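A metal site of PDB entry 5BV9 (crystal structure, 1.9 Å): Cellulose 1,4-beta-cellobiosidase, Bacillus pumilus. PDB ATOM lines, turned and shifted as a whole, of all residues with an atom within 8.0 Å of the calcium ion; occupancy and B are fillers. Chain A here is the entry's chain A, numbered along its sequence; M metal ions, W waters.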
ATOM      1  N   PRO A 112      13.033 -33.884   6.001  1.00  0.00           N
ATOM      2  CA  PRO A 112      12.881 -32.421   5.980  1.00  0.00           C
ATOM      3  C   PRO A 112      12.207 -31.811   7.233  1.00  0.00           C
ATOM      4  O   PRO A 112      12.304 -30.573   7.416  1.00  0.00           O
ATOM      5  CB  PRO A 112      12.012 -32.166   4.768  1.00  0.00           C
ATOM      6  CG  PRO A 112      11.304 -33.450   4.490  1.00  0.00           C
ATOM      7  CD  PRO A 112      12.137 -34.556   5.049  1.00  0.00           C
ATOM      8  N   TYR A 113      11.510 -32.646   8.011  1.00  0.00           N
ATOM      9  CA  TYR A 113      10.948 -32.238   9.327  1.00  0.00           C
ATOM     10  C   TYR A 113      11.180 -33.266  10.398  1.00  0.00           C
ATOM     11  O   TYR A 113      11.185 -34.429  10.079  1.00  0.00           O
ATOM     12  CB  TYR A 113       9.412 -32.061   9.255  1.00  0.00           C
ATOM     13  CG  TYR A 113       9.084 -30.959   8.275  1.00  0.00           C
ATOM     14  CD1 TYR A 113       9.218 -29.623   8.620  1.00  0.00           C
ATOM     15  CD2 TYR A 113       8.706 -31.277   6.966  1.00  0.00           C
ATOM     16  CE1 TYR A 113       9.007 -28.606   7.673  1.00  0.00           C
ATOM     17  CE2 TYR A 113       8.405 -30.272   6.042  1.00  0.00           C
ATOM     18  CZ  TYR A 113       8.557 -28.945   6.409  1.00  0.00           C
ATOM     19  OH  TYR A 113       8.295 -27.996   5.427  1.00  0.00           O
ATOM     20  N   PRO A 114      11.361 -32.841  11.657  1.00  0.00           N
ATOM     21  CA  PRO A 114      11.457 -33.806  12.724  1.00  0.00           C
ATOM     22  C   PRO A 114      10.297 -34.781  12.824  1.00  0.00           C
ATOM     23  O   PRO A 114      10.504 -35.915  13.248  1.00  0.00           O
ATOM     24  CB  PRO A 114      11.481 -32.958  13.961  1.00  0.00           C
ATOM     25  CG  PRO A 114      11.848 -31.572  13.527  1.00  0.00           C
ATOM     26  CD  PRO A 114      11.281 -31.462  12.169  1.00  0.00           C
ATOM     27  N   ASP A 115       9.106 -34.324  12.393  1.00  0.00           N
ATOM     28  CA  ASP A 115       7.904 -35.126  12.323  1.00  0.00           C
ATOM     29  C   ASP A 115       8.025 -36.418  11.579  1.00  0.00           C
ATOM     30  O   ASP A 115       7.258 -37.322  11.826  1.00  0.00           O
ATOM     31  CB  ASP A 115       6.740 -34.332  11.674  1.00  0.00           C
ATOM     32  CG  ASP A 115       6.600 -32.914  12.207  1.00  0.00           C
ATOM     33  OD1 ASP A 115       7.655 -32.171  12.216  1.00  0.00           O
ATOM     34  OD2 ASP A 115       5.464 -32.543  12.509  1.00  0.00           O
ATOM     35  N   GLY A 179      17.269 -33.793  11.551  1.00  0.00           N
ATOM     36  CA  GLY A 179      17.275 -33.084  10.275  1.00  0.00           C
ATOM     37  C   GLY A 179      17.281 -31.594  10.380  1.00  0.00           C
ATOM     38  O   GLY A 179      17.375 -30.978  11.494  1.00  0.00           O
ATOM     39  N   GLN A 180      17.088 -30.977   9.213  1.00  0.00           N
ATOM     40  CA  GLN A 180      17.324 -29.586   9.009  1.00  0.00           C
ATOM     41  C   GLN A 180      16.368 -28.670   9.704  1.00  0.00           C
ATOM     42  O   GLN A 180      16.724 -27.492   9.939  1.00  0.00           O
ATOM     43  CB  GLN A 180      17.349 -29.273   7.504  1.00  0.00           C
ATOM     44  CG  GLN A 180      16.000 -29.395   6.803  1.00  0.00           C
ATOM     45  CD  GLN A 180      16.176 -29.520   5.289  1.00  0.00           C
ATOM     46  OE1 GLN A 180      17.272 -29.690   4.810  1.00  0.00           O
ATOM     47  NE2 GLN A 180      15.113 -29.403   4.564  1.00  0.00           N
ATOM     48  N   GLN A 181      15.168 -29.161   9.962  1.00  0.00           N
ATOM     49  CA  GLN A 181      14.172 -28.340  10.657  1.00  0.00           C
ATOM     50  C   GLN A 181      14.128 -28.519  12.161  1.00  0.00           C
ATOM     51  O   GLN A 181      13.264 -27.948  12.840  1.00  0.00           O
ATOM     52  CB  GLN A 181      12.793 -28.542  10.046  1.00  0.00           C
ATOM     53  CG  GLN A 181      12.430 -27.564   8.947  1.00  0.00           C
ATOM     54  CD  GLN A 181      12.370 -26.110   9.467  1.00  0.00           C
ATOM     55  OE1 GLN A 181      12.075 -25.851  10.605  1.00  0.00           O
ATOM     56  NE2 GLN A 181      12.635 -25.183   8.586  1.00  0.00           N
ATOM     57  N   GLU A 182      15.023 -29.301  12.742  1.00  0.00           N
ATOM     58  CA  GLU A 182      14.977 -29.427  14.182  1.00  0.00           C
ATOM     59  C   GLU A 182      15.786 -28.290  14.768  1.00  0.00           C
ATOM     60  O   GLU A 182      17.014 -28.399  14.852  1.00  0.00           O
ATOM     61  CB  GLU A 182      15.609 -30.766  14.612  1.00  0.00           C
ATOM     62  CG  GLU A 182      15.428 -31.062  16.120  1.00  0.00           C
ATOM     63  CD  GLU A 182      15.995 -32.373  16.531  1.00  0.00           C
ATOM     64  OE1 GLU A 182      17.145 -32.676  16.129  1.00  0.00           O
ATOM     65  OE2 GLU A 182      15.284 -33.080  17.214  1.00  0.00           O
ATOM     66  N   SER A 183      15.144 -27.193  15.126  1.00  0.00           N
ATOM     67  CA  SER A 183      15.856 -26.112  15.813  1.00  0.00           C
ATOM     68  C   SER A 183      16.303 -26.557  17.189  1.00  0.00           C
ATOM     69  O   SER A 183      15.860 -27.593  17.702  1.00  0.00           O
ATOM     70  CB  SER A 183      14.982 -24.856  15.958  1.00  0.00           C
ATOM     71  OG  SER A 183      13.952 -25.059  16.952  1.00  0.00           O
ATOM     72  N   VAL A 184      17.063 -25.694  17.849  1.00  0.00           N
ATOM     73  CA  VAL A 184      17.481 -25.951  19.227  1.00  0.00           C
ATOM     74  C   VAL A 184      16.235 -26.145  20.139  1.00  0.00           C
ATOM     75  O   VAL A 184      16.193 -27.014  21.070  1.00  0.00           O
ATOM     76  CB  VAL A 184      18.425 -24.850  19.774  1.00  0.00           C
ATOM     77  CG1 VAL A 184      17.739 -23.474  19.812  1.00  0.00           C
ATOM     78  CG2 VAL A 184      18.890 -25.201  21.168  1.00  0.00           C
ATOM     79  N   TRP A 185      15.180 -25.453  19.801  1.00  0.00           N
ATOM     80  CA  TRP A 185      13.916 -25.525  20.567  1.00  0.00           C
ATOM     81  C   TRP A 185      13.144 -26.815  20.366  1.00  0.00           C
ATOM     82  O   TRP A 185      12.240 -27.138  21.137  1.00  0.00           O
ATOM     83  CB  TRP A 185      12.999 -24.369  20.112  1.00  0.00           C
ATOM     84  CG  TRP A 185      13.665 -23.090  20.183  1.00  0.00           C
ATOM     85  CD1 TRP A 185      14.220 -22.361  19.149  1.00  0.00           C
ATOM     86  CD2 TRP A 185      13.867 -22.328  21.350  1.00  0.00           C
ATOM     87  NE1 TRP A 185      14.751 -21.177  19.638  1.00  0.00           N
ATOM     88  CE2 TRP A 185      14.578 -21.162  21.002  1.00  0.00           C
ATOM     89  CE3 TRP A 185      13.498 -22.515  22.696  1.00  0.00           C
ATOM     90  CZ2 TRP A 185      14.872 -20.188  21.921  1.00  0.00           C
ATOM     91  CZ3 TRP A 185      13.895 -21.604  23.600  1.00  0.00           C
ATOM     92  CH2 TRP A 185      14.551 -20.436  23.209  1.00  0.00           C
ATOM     93  N   GLU A 186      13.451 -27.512  19.296  1.00  0.00           N
ATOM     94  CA  GLU A 186      12.678 -28.707  18.859  1.00  0.00           C
ATOM     95  C   GLU A 186      13.363 -30.037  19.155  1.00  0.00           C
ATOM     96  O   GLU A 186      12.795 -31.116  18.829  1.00  0.00           O
ATOM     97  CB  GLU A 186      12.392 -28.540  17.389  1.00  0.00           C
ATOM     98  CG  GLU A 186      11.436 -27.386  17.086  1.00  0.00           C
ATOM     99  CD  GLU A 186      11.462 -27.075  15.625  1.00  0.00           C
ATOM    100  OE1 GLU A 186      10.674 -27.638  14.866  1.00  0.00           O
ATOM    101  OE2 GLU A 186      12.333 -26.320  15.216  1.00  0.00           O
ATOM    102  N   HIS A 404      18.208 -25.174   9.019  1.00  0.00           N
ATOM    103  CA  HIS A 404      17.379 -24.208   8.398  1.00  0.00           C
ATOM    104  C   HIS A 404      16.539 -23.400   9.369  1.00  0.00           C
ATOM    105  O   HIS A 404      15.858 -22.458   8.925  1.00  0.00           O
ATOM    106  CB  HIS A 404      16.399 -24.927   7.462  1.00  0.00           C
ATOM    107  CG  HIS A 404      17.046 -25.504   6.257  1.00  0.00           C
ATOM    108  ND1 HIS A 404      16.336 -26.066   5.237  1.00  0.00           N
ATOM    109  CD2 HIS A 404      18.343 -25.620   5.913  1.00  0.00           C
ATOM    110  CE1 HIS A 404      17.154 -26.467   4.296  1.00  0.00           C
ATOM    111  NE2 HIS A 404      18.388 -26.207   4.692  1.00  0.00           N
ATOM    112  N   ASP A 405      16.636 -23.691  10.668  1.00  0.00           N
ATOM    113  CA  ASP A 405      15.782 -22.995  11.645  1.00  0.00           C
ATOM    114  C   ASP A 405      16.632 -22.524  12.814  1.00  0.00           C
ATOM    115  O   ASP A 405      16.762 -23.247  13.810  1.00  0.00           O
ATOM    116  CB  ASP A 405      14.645 -23.962  12.040  1.00  0.00           C
ATOM    117  CG  ASP A 405      13.555 -23.323  12.873  1.00  0.00           C
ATOM    118  OD1 ASP A 405      13.622 -22.119  13.216  1.00  0.00           O
ATOM    119  OD2 ASP A 405      12.651 -24.101  13.241  1.00  0.00           O
ATOM    120  N   PRO A 406      17.268 -21.351  12.732  1.00  0.00           N
ATOM    121  CA  PRO A 406      17.264 -20.422  11.617  1.00  0.00           C
ATOM    122  C   PRO A 406      18.320 -20.917  10.533  1.00  0.00           C
ATOM    123  O   PRO A 406      19.220 -21.742  10.852  1.00  0.00           O
ATOM    124  CB  PRO A 406      17.745 -19.139  12.265  1.00  0.00           C
ATOM    125  CG  PRO A 406      18.714 -19.584  13.326  1.00  0.00           C
ATOM    126  CD  PRO A 406      18.182 -20.902  13.810  1.00  0.00           C
ATOM    127  N   ARG A 597       9.631 -19.318  21.880  1.00  0.00           N
ATOM    128  CA  ARG A 597       9.794 -20.781  21.628  1.00  0.00           C
ATOM    129  C   ARG A 597      10.107 -21.657  22.863  1.00  0.00           C
ATOM    130  O   ARG A 597      10.133 -22.896  22.795  1.00  0.00           O
ATOM    131  CB  ARG A 597      10.822 -20.955  20.513  1.00  0.00           C
ATOM    132  CG  ARG A 597      10.386 -20.186  19.255  1.00  0.00           C
ATOM    133  CD  ARG A 597      11.355 -20.446  18.118  1.00  0.00           C
ATOM    134  NE  ARG A 597      11.102 -21.754  17.467  1.00  0.00           N
ATOM    135  CZ  ARG A 597      11.716 -22.215  16.385  1.00  0.00           C
ATOM    136  NH1 ARG A 597      11.399 -23.432  15.896  1.00  0.00           N
ATOM    137  NH2 ARG A 597      12.609 -21.467  15.747  1.00  0.00           N
ATOM    138  N   GLU A 602       5.876 -27.245  19.824  1.00  0.00           N
ATOM    139  CA  GLU A 602       6.567 -27.616  18.622  1.00  0.00           C
ATOM    140  C   GLU A 602       7.644 -28.656  18.836  1.00  0.00           C
ATOM    141  O   GLU A 602       8.398 -28.929  17.916  1.00  0.00           O
ATOM    142  CB  GLU A 602       7.169 -26.370  17.917  1.00  0.00           C
ATOM    143  CG  GLU A 602       7.216 -26.567  16.409  1.00  0.00           C
ATOM    144  CD  GLU A 602       7.692 -25.357  15.650  1.00  0.00           C
ATOM    145  OE1 GLU A 602       7.400 -25.303  14.428  1.00  0.00           O
ATOM    146  OE2 GLU A 602       8.333 -24.490  16.267  1.00  0.00           O
ATOM    147  N   ARG A 631       3.742 -31.558   7.653  1.00  0.00           N
ATOM    148  CA  ARG A 631       5.123 -31.959   7.874  1.00  0.00           C
ATOM    149  C   ARG A 631       5.332 -33.408   7.810  1.00  0.00           C
ATOM    150  O   ARG A 631       6.435 -33.878   8.080  1.00  0.00           O
ATOM    151  CB  ARG A 631       5.607 -31.443   9.194  1.00  0.00           C
ATOM    152  CG  ARG A 631       5.424 -29.931   9.239  1.00  0.00           C
ATOM    153  CD  ARG A 631       6.065 -29.291  10.448  1.00  0.00           C
ATOM    154  NE  ARG A 631       5.750 -27.881  10.448  1.00  0.00           N
ATOM    155  CZ  ARG A 631       5.971 -27.036  11.445  1.00  0.00           C
ATOM    156  NH1 ARG A 631       6.550 -27.430  12.562  1.00  0.00           N
ATOM    157  NH2 ARG A 631       5.625 -25.766  11.307  1.00  0.00           N
HETATM  158 CA    CA M   1      11.643 -26.187  12.870  1.00  0.00          CA
HETATM  159  O   HOH W   1       9.740 -24.921  13.010  1.00  0.00           O
HETATM  160  O   HOH W   2       9.983 -27.968  11.907  1.00  0.00           O
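Of the 18 residues printed, 3 come within 4 Å of the calcium ion. The nearest printed residue that does not touch the calcium ion is Arg 597 (4.1 Å).
The calcium ion is bound by water W1 (2.3 Å), the side-chain amide oxygen (OE1) of Gln 181 (2.3 Å), the side-chain carboxylate (OD2) of Asp 405 (2.3 Å), the backbone carbonyl oxygen (O) of Gln 181 (2.4 Å), the side-chain carboxylate (OE2) of Glu 186 (2.4 Å), water W2 (2.6 Å) and the side-chain carboxylate (OE1) of Glu 186 (2.7 Å).
The guanidinium group (NH2) of Arg 597 is in salt-bridge range of the side-chain carboxylate (OD1) of Asp 405 (2.8 Å). NH1 of Arg 597 sits close to OE2 of Glu 186, at 3.1 Å. The side-chain hydroxyl of Ser 183 lies close to the backbone NH of Glu 186.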
